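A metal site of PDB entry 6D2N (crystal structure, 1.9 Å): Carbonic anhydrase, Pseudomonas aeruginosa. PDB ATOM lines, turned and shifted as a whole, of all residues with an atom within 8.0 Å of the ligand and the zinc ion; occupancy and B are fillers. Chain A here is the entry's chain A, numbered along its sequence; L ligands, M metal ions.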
ATOM      1  N   GLY A  39      32.690  11.346 -12.661  1.00  0.00           N
ATOM      2  CA  GLY A  39      31.496  11.104 -11.885  1.00  0.00           C
ATOM      3  C   GLY A  39      30.774  12.383 -11.556  1.00  0.00           C
ATOM      4  O   GLY A  39      31.195  13.444 -12.001  1.00  0.00           O
ATOM      5  N   CYS A  40      29.693  12.284 -10.780  1.00  0.00           N
ATOM      6  CA  CYS A  40      28.943  13.476 -10.369  1.00  0.00           C
ATOM      7  C   CYS A  40      29.596  14.207  -9.201  1.00  0.00           C
ATOM      8  O   CYS A  40      30.300  13.602  -8.403  1.00  0.00           O
ATOM      9  CB  CYS A  40      27.499  13.124  -9.986  1.00  0.00           C
ATOM     10  SG  CYS A  40      26.415  14.587  -9.709  1.00  0.00           S
ATOM     11  N   SER A  41      29.331  15.508  -9.093  1.00  0.00           N
ATOM     12  CA  SER A  41      29.818  16.357  -8.004  1.00  0.00           C
ATOM     13  C   SER A  41      29.086  16.068  -6.670  1.00  0.00           C
ATOM     14  O   SER A  41      29.553  16.475  -5.612  1.00  0.00           O
ATOM     15  CB  SER A  41      29.620  17.831  -8.371  1.00  0.00           C
ATOM     16  OG  SER A  41      30.436  18.180  -9.484  1.00  0.00           O
ATOM     17  N   ASP A  42      27.941  15.420  -6.769  1.00  0.00           N
ATOM     18  CA  ASP A  42      27.127  15.036  -5.619  1.00  0.00           C
ATOM     19  C   ASP A  42      28.010  14.570  -4.442  1.00  0.00           C
ATOM     20  O   ASP A  42      28.887  13.703  -4.606  1.00  0.00           O
ATOM     21  CB  ASP A  42      26.152  13.928  -6.038  1.00  0.00           C
ATOM     22  CG  ASP A  42      25.109  13.610  -4.977  1.00  0.00           C
ATOM     23  OD1 ASP A  42      23.900  13.527  -5.313  1.00  0.00           O
ATOM     24  OD2 ASP A  42      25.505  13.459  -3.796  1.00  0.00           O
ATOM     25  N   ALA A  43      27.794  15.157  -3.269  1.00  0.00           N
ATOM     26  CA  ALA A  43      28.647  14.949  -2.092  1.00  0.00           C
ATOM     27  C   ALA A  43      28.577  13.516  -1.600  1.00  0.00           C
ATOM     28  O   ALA A  43      29.420  13.069  -0.796  1.00  0.00           O
ATOM     29  CB  ALA A  43      28.265  15.912  -0.992  1.00  0.00           C
ATOM     30  N   ARG A  44      27.551  12.815  -2.046  1.00  0.00           N
ATOM     31  CA  ARG A  44      27.308  11.451  -1.579  1.00  0.00           C
ATOM     32  C   ARG A  44      28.058  10.427  -2.418  1.00  0.00           C
ATOM     33  O   ARG A  44      28.005   9.237  -2.131  1.00  0.00           O
ATOM     34  CB  ARG A  44      25.804  11.168  -1.605  1.00  0.00           C
ATOM     35  CG  ARG A  44      25.017  11.979  -0.559  1.00  0.00           C
ATOM     36  CD  ARG A  44      23.518  11.945  -0.834  1.00  0.00           C
ATOM     37  NE  ARG A  44      23.192  12.595  -2.105  1.00  0.00           N
ATOM     38  CZ  ARG A  44      21.957  12.830  -2.511  1.00  0.00           C
ATOM     39  NH1 ARG A  44      20.951  12.469  -1.724  1.00  0.00           N
ATOM     40  NH2 ARG A  44      21.729  13.427  -3.680  1.00  0.00           N
ATOM     41  N   VAL A  45      28.783  10.899  -3.437  1.00  0.00           N
ATOM     42  CA  VAL A  45      29.503  10.011  -4.349  1.00  0.00           C
ATOM     43  C   VAL A  45      31.030  10.281  -4.399  1.00  0.00           C
ATOM     44  O   VAL A  45      31.579  10.536  -5.468  1.00  0.00           O
ATOM     45  CB  VAL A  45      28.885  10.044  -5.786  1.00  0.00           C
ATOM     46  CG1 VAL A  45      29.264   8.809  -6.591  1.00  0.00           C
ATOM     47  CG2 VAL A  45      27.366  10.115  -5.711  1.00  0.00           C
ATOM     48  N   ASN A  63      31.620  16.565 -12.215  1.00  0.00           N
ATOM     49  CA  ASN A  63      30.783  17.696 -12.632  1.00  0.00           C
ATOM     50  C   ASN A  63      29.294  17.372 -12.368  1.00  0.00           C
ATOM     51  O   ASN A  63      28.966  16.240 -11.980  1.00  0.00           O
ATOM     52  CB  ASN A  63      31.067  18.078 -14.111  1.00  0.00           C
ATOM     53  CG  ASN A  63      30.565  17.027 -15.114  1.00  0.00           C
ATOM     54  OD1 ASN A  63      29.427  16.589 -15.069  1.00  0.00           O
ATOM     55  ND2 ASN A  63      31.421  16.684 -16.098  1.00  0.00           N
ATOM     56  N   VAL A  64      28.398  18.332 -12.592  1.00  0.00           N
ATOM     57  CA  VAL A  64      26.974  18.026 -12.368  1.00  0.00           C
ATOM     58  C   VAL A  64      26.469  16.991 -13.371  1.00  0.00           C
ATOM     59  O   VAL A  64      26.412  17.243 -14.594  1.00  0.00           O
ATOM     60  CB  VAL A  64      26.071  19.253 -12.418  1.00  0.00           C
ATOM     61  CG1 VAL A  64      24.621  18.796 -12.279  1.00  0.00           C
ATOM     62  CG2 VAL A  64      26.420  20.213 -11.296  1.00  0.00           C
ATOM     63  N   ALA A  65      26.103  15.834 -12.832  1.00  0.00           N
ATOM     64  CA  ALA A  65      25.563  14.692 -13.581  1.00  0.00           C
ATOM     65  C   ALA A  65      26.555  14.039 -14.537  1.00  0.00           C
ATOM     66  O   ALA A  65      26.144  13.360 -15.500  1.00  0.00           O
ATOM     67  CB  ALA A  65      24.289  15.087 -14.325  1.00  0.00           C
ATOM     68  N   ASN A  66      27.837  14.176 -14.242  1.00  0.00           N
ATOM     69  CA  ASN A  66      28.882  13.430 -14.965  1.00  0.00           C
ATOM     70  C   ASN A  66      28.689  13.461 -16.485  1.00  0.00           C
ATOM     71  O   ASN A  66      28.630  12.419 -17.159  1.00  0.00           O
ATOM     72  CB  ASN A  66      29.042  11.983 -14.434  1.00  0.00           C
ATOM     73  CG  ASN A  66      27.724  11.199 -14.404  1.00  0.00           C
ATOM     74  OD1 ASN A  66      27.339  10.565 -15.390  1.00  0.00           O
ATOM     75  ND2 ASN A  66      27.041  11.218 -13.263  1.00  0.00           N
ATOM     76  N   THR A  94      31.238   6.897 -13.847  1.00  0.00           N
ATOM     77  CA  THR A  94      30.299   6.499 -12.816  1.00  0.00           C
ATOM     78  C   THR A  94      29.193   7.537 -12.631  1.00  0.00           C
ATOM     79  O   THR A  94      29.434   8.659 -12.165  1.00  0.00           O
ATOM     80  CB  THR A  94      31.023   6.297 -11.470  1.00  0.00           C
ATOM     81  OG1 THR A  94      32.080   5.350 -11.631  1.00  0.00           O
ATOM     82  CG2 THR A  94      30.049   5.804 -10.385  1.00  0.00           C
ATOM     83  N   GLY A  95      27.969   7.158 -12.983  1.00  0.00           N
ATOM     84  CA  GLY A  95      26.822   8.006 -12.662  1.00  0.00           C
ATOM     85  C   GLY A  95      26.301   7.496 -11.330  1.00  0.00           C
ATOM     86  O   GLY A  95      26.976   6.676 -10.687  1.00  0.00           O
ATOM     87  N   HIS A  96      25.136   7.965 -10.908  1.00  0.00           N
ATOM     88  CA  HIS A  96      24.535   7.395  -9.687  1.00  0.00           C
ATOM     89  C   HIS A  96      23.023   7.509  -9.683  1.00  0.00           C
ATOM     90  O   HIS A  96      22.441   8.351 -10.368  1.00  0.00           O
ATOM     91  CB  HIS A  96      25.135   8.028  -8.427  1.00  0.00           C
ATOM     92  CG  HIS A  96      24.862   9.503  -8.307  1.00  0.00           C
ATOM     93  ND1 HIS A  96      23.856  10.021  -7.516  1.00  0.00           N
ATOM     94  CD2 HIS A  96      25.463  10.567  -8.889  1.00  0.00           C
ATOM     95  CE1 HIS A  96      23.849  11.333  -7.618  1.00  0.00           C
ATOM     96  NE2 HIS A  96      24.823  11.695  -8.434  1.00  0.00           N
ATOM     97  N   TYR A  97      22.371   6.640  -8.906  1.00  0.00           N
ATOM     98  CA  TYR A  97      20.924   6.711  -8.760  1.00  0.00           C
ATOM     99  C   TYR A  97      20.517   7.924  -7.915  1.00  0.00           C
ATOM    100  O   TYR A  97      21.294   8.380  -7.065  1.00  0.00           O
ATOM    101  CB  TYR A  97      20.380   5.406  -8.174  1.00  0.00           C
ATOM    102  CG  TYR A  97      20.541   4.205  -9.081  1.00  0.00           C
ATOM    103  CD1 TYR A  97      21.340   3.133  -8.715  1.00  0.00           C
ATOM    104  CD2 TYR A  97      19.906   4.157 -10.323  1.00  0.00           C
ATOM    105  CE1 TYR A  97      21.492   2.023  -9.556  1.00  0.00           C
ATOM    106  CE2 TYR A  97      20.056   3.053 -11.172  1.00  0.00           C
ATOM    107  CZ  TYR A  97      20.849   1.991 -10.785  1.00  0.00           C
ATOM    108  OH  TYR A  97      21.002   0.911 -11.631  1.00  0.00           O
ATOM    109  N   GLY A  98      19.323   8.464  -8.169  1.00  0.00           N
ATOM    110  CA  GLY A  98      18.876   9.635  -7.430  1.00  0.00           C
ATOM    111  C   GLY A  98      19.636  10.917  -7.783  1.00  0.00           C
ATOM    112  O   GLY A  98      19.643  11.891  -7.022  1.00  0.00           O
ATOM    113  N   CYS A  99      20.274  10.925  -8.957  1.00  0.00           N
ATOM    114  CA  CYS A  99      21.019  12.117  -9.394  1.00  0.00           C
ATOM    115  C   CYS A  99      20.104  13.320  -9.607  1.00  0.00           C
ATOM    116  O   CYS A  99      19.140  13.242 -10.377  1.00  0.00           O
ATOM    117  CB  CYS A  99      21.790  11.833 -10.690  1.00  0.00           C
ATOM    118  SG  CYS A  99      22.921  13.187 -11.236  1.00  0.00           S
ATOM    119  N   GLY A 100      20.425  14.431  -8.943  1.00  0.00           N
ATOM    120  CA  GLY A 100      19.604  15.632  -9.005  1.00  0.00           C
ATOM    121  C   GLY A 100      19.692  16.354 -10.342  1.00  0.00           C
ATOM    122  O   GLY A 100      18.714  16.962 -10.780  1.00  0.00           O
ATOM    123  N   GLY A 101      20.862  16.262 -10.985  1.00  0.00           N
ATOM    124  CA  GLY A 101      21.011  16.791 -12.333  1.00  0.00           C
ATOM    125  C   GLY A 101      20.112  16.057 -13.301  1.00  0.00           C
ATOM    126  O   GLY A 101      19.439  16.668 -14.139  1.00  0.00           O
ATOM    127  N   VAL A 102      20.088  14.722 -13.184  1.00  0.00           N
ATOM    128  CA  VAL A 102      19.253  13.898 -14.029  1.00  0.00           C
ATOM    129  C   VAL A 102      17.784  14.205 -13.765  1.00  0.00           C
ATOM    130  O   VAL A 102      17.012  14.419 -14.696  1.00  0.00           O
ATOM    131  CB  VAL A 102      19.532  12.404 -13.829  1.00  0.00           C
ATOM    132  CG1 VAL A 102      18.474  11.565 -14.550  1.00  0.00           C
ATOM    133  CG2 VAL A 102      20.920  12.050 -14.344  1.00  0.00           C
ATOM    134  N   ARG A 103      17.413  14.248 -12.490  1.00  0.00           N
ATOM    135  CA  ARG A 103      16.035  14.523 -12.095  1.00  0.00           C
ATOM    136  C   ARG A 103      15.548  15.855 -12.634  1.00  0.00           C
ATOM    137  O   ARG A 103      14.417  15.945 -13.115  1.00  0.00           O
ATOM    138  CB  ARG A 103      15.894  14.505 -10.567  1.00  0.00           C
ATOM    139  CG  ARG A 103      14.463  14.705 -10.039  1.00  0.00           C
ATOM    140  CD  ARG A 103      14.342  14.444  -8.523  1.00  0.00           C
ATOM    141  NE  ARG A 103      14.313  13.018  -8.183  1.00  0.00           N
ATOM    142  CZ  ARG A 103      15.308  12.371  -7.577  1.00  0.00           C
ATOM    143  NH1 ARG A 103      16.432  13.008  -7.271  1.00  0.00           N
ATOM    144  NH2 ARG A 103      15.193  11.077  -7.287  1.00  0.00           N
ATOM    145  N   ALA A 104      16.386  16.884 -12.562  1.00  0.00           N
ATOM    146  CA  ALA A 104      15.994  18.226 -13.003  1.00  0.00           C
ATOM    147  C   ALA A 104      15.798  18.274 -14.523  1.00  0.00           C
ATOM    148  O   ALA A 104      15.029  19.088 -15.037  1.00  0.00           O
ATOM    149  CB  ALA A 104      17.028  19.245 -12.573  1.00  0.00           C
ATOM    150  N   ILE A 114      22.720  25.931 -15.170  1.00  0.00           N
ATOM    151  CA  ILE A 114      22.763  24.480 -15.235  1.00  0.00           C
ATOM    152  C   ILE A 114      21.784  23.921 -16.262  1.00  0.00           C
ATOM    153  O   ILE A 114      21.951  22.781 -16.719  1.00  0.00           O
ATOM    154  CB  ILE A 114      22.495  23.861 -13.862  1.00  0.00           C
ATOM    155  CG1 ILE A 114      23.013  22.433 -13.829  1.00  0.00           C
ATOM    156  CG2 ILE A 114      21.028  23.881 -13.574  1.00  0.00           C
ATOM    157  CD1 ILE A 114      23.336  21.980 -12.458  1.00  0.00           C
ATOM    158  N   LEU A 118      22.723  20.609 -18.608  1.00  0.00           N
ATOM    159  CA  LEU A 118      21.960  19.363 -18.526  1.00  0.00           C
ATOM    160  C   LEU A 118      21.208  19.044 -19.819  1.00  0.00           C
ATOM    161  O   LEU A 118      20.549  18.016 -19.905  1.00  0.00           O
ATOM    162  CB  LEU A 118      20.950  19.479 -17.382  1.00  0.00           C
ATOM    163  CG  LEU A 118      21.557  19.649 -15.987  1.00  0.00           C
ATOM    164  CD1 LEU A 118      20.453  19.790 -14.952  1.00  0.00           C
ATOM    165  CD2 LEU A 118      22.455  18.466 -15.694  1.00  0.00           C
ATOM    166  N   ILE A 121      21.143  15.575 -21.298  1.00  0.00           N
ATOM    167  CA  ILE A 121      20.357  14.590 -20.560  1.00  0.00           C
ATOM    168  C   ILE A 121      18.887  14.796 -20.910  1.00  0.00           C
ATOM    169  O   ILE A 121      18.118  13.837 -20.961  1.00  0.00           O
ATOM    170  CB  ILE A 121      20.537  14.715 -19.040  1.00  0.00           C
ATOM    171  CG1 ILE A 121      22.018  14.704 -18.669  1.00  0.00           C
ATOM    172  CG2 ILE A 121      19.816  13.565 -18.294  1.00  0.00           C
ATOM    173  CD1 ILE A 121      22.273  14.842 -17.169  1.00  0.00           C
ATOM    174  N   CYS A 146      19.323   7.844 -15.256  1.00  0.00           N
ATOM    175  CA  CYS A 146      20.674   7.868 -14.683  1.00  0.00           C
ATOM    176  C   CYS A 146      21.566   6.850 -15.388  1.00  0.00           C
ATOM    177  O   CYS A 146      22.711   7.150 -15.754  1.00  0.00           O
ATOM    178  CB  CYS A 146      20.633   7.597 -13.179  1.00  0.00           C
ATOM    179  SG  CYS A 146      20.083   9.018 -12.170  1.00  0.00           S
ATOM    180  N   ASN A 149      22.080   7.757 -19.065  1.00  0.00           N
ATOM    181  CA  ASN A 149      23.065   8.830 -19.119  1.00  0.00           C
ATOM    182  C   ASN A 149      24.489   8.302 -19.056  1.00  0.00           C
ATOM    183  O   ASN A 149      25.336   8.683 -19.881  1.00  0.00           O
ATOM    184  CB  ASN A 149      22.822   9.864 -18.013  1.00  0.00           C
ATOM    185  CG  ASN A 149      23.772  11.030 -18.105  1.00  0.00           C
ATOM    186  OD1 ASN A 149      24.017  11.562 -19.201  1.00  0.00           O
ATOM    187  ND2 ASN A 149      24.327  11.434 -16.969  1.00  0.00           N
ATOM    188  N   ILE A 182      23.261   5.539  -4.138  1.00  0.00           N
ATOM    189  CA  ILE A 182      23.376   6.329  -2.910  1.00  0.00           C
ATOM    190  C   ILE A 182      22.550   5.726  -1.761  1.00  0.00           C
ATOM    191  O   ILE A 182      22.721   6.110  -0.604  1.00  0.00           O
ATOM    192  CB  ILE A 182      23.005   7.819  -3.105  1.00  0.00           C
ATOM    193  CG1 ILE A 182      21.601   7.967  -3.694  1.00  0.00           C
ATOM    194  CG2 ILE A 182      24.059   8.529  -3.957  1.00  0.00           C
ATOM    195  CD1 ILE A 182      21.128   9.422  -3.805  1.00  0.00           C
HETATM  196  N1  LIG L   1      21.971  16.671  -7.258  1.00  0.00           N
HETATM  197  S1  LIG L   1      23.341  16.158  -8.002  1.00  0.00           S
HETATM  198  O1  LIG L   1      24.491  16.909  -7.388  1.00  0.00           O
HETATM  199  O2  LIG L   1      23.290  16.430  -9.485  1.00  0.00           O
HETATM  200  N2  LIG L   1      23.543  14.528  -7.880  1.00  0.00           N
HETATM  201 ZN    ZN M   1      24.371  13.569  -9.409  1.00  0.00          ZN
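The side-chain carboxylate (OD1) of Asp 42 lies close to a nitrogen (N2) of the ligand, at 2.8 Å. O2 of the ligand lies within hydrogen-bond range of N of Gly 101, 2.9 Å away.
The side-chain carboxylate of Asp 42 lies within salt-bridge range of the guanidinium group of Arg 44 (2.7 Å). The backbone carbonyl oxygen (O) of His 96 sits at hydrogen-bond distance from the side-chain sulfur (SG) of Cys 146 (3.0 Å). N of Val 102 sits close to SG of Cys 99, at 3.8 Å. The backbone NH (N) of Cys 99 sits close to the side-chain sulfur (SG) of Cys 146, 3.7 Å away. O of Asn 63 sits close to SG of Cys 40. The backbone NH (N) of Ala 65 sits close to the side-chain sulfur (SG) of Cys 40 (3.4 Å). The backbone NH (N) of Gly 101 sits close to the side-chain sulfur (SG) of Cys 99, 3.7 Å away. SG of Cys 40 lies close to N of Asp 42, 3.4 Å away.
Residues that only touch the zinc ion: Asp 42 (3.8 Å). Within 4 Å of the zinc ion: Cys 40, Asp 42, His 96 and Cys 99. The nearest printed residue that does not touch the zinc ion is Gly 100 (4.1 Å).
N of Gly 100 sits close to N1 of the ligand (3.2 Å). Residues that only touch the ligand: Val 64 (3.9 Å). Hydrophobic or aromatic side chains within 4 Å of the ligand: Val 64 and His 96. Of the 28 residues printed, 7 come within 4 Å of the ligand.
A nitrogen (N2) of the ligand binds the zinc ion, at 2.0 Å. NE2 of His 96 binds the zinc ion, 2.2 Å away. SG of Cys 40 is bound to the zinc ion, 2.3 Å away. The zinc ion is bound by SG of Cys 99 (2.4 Å).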
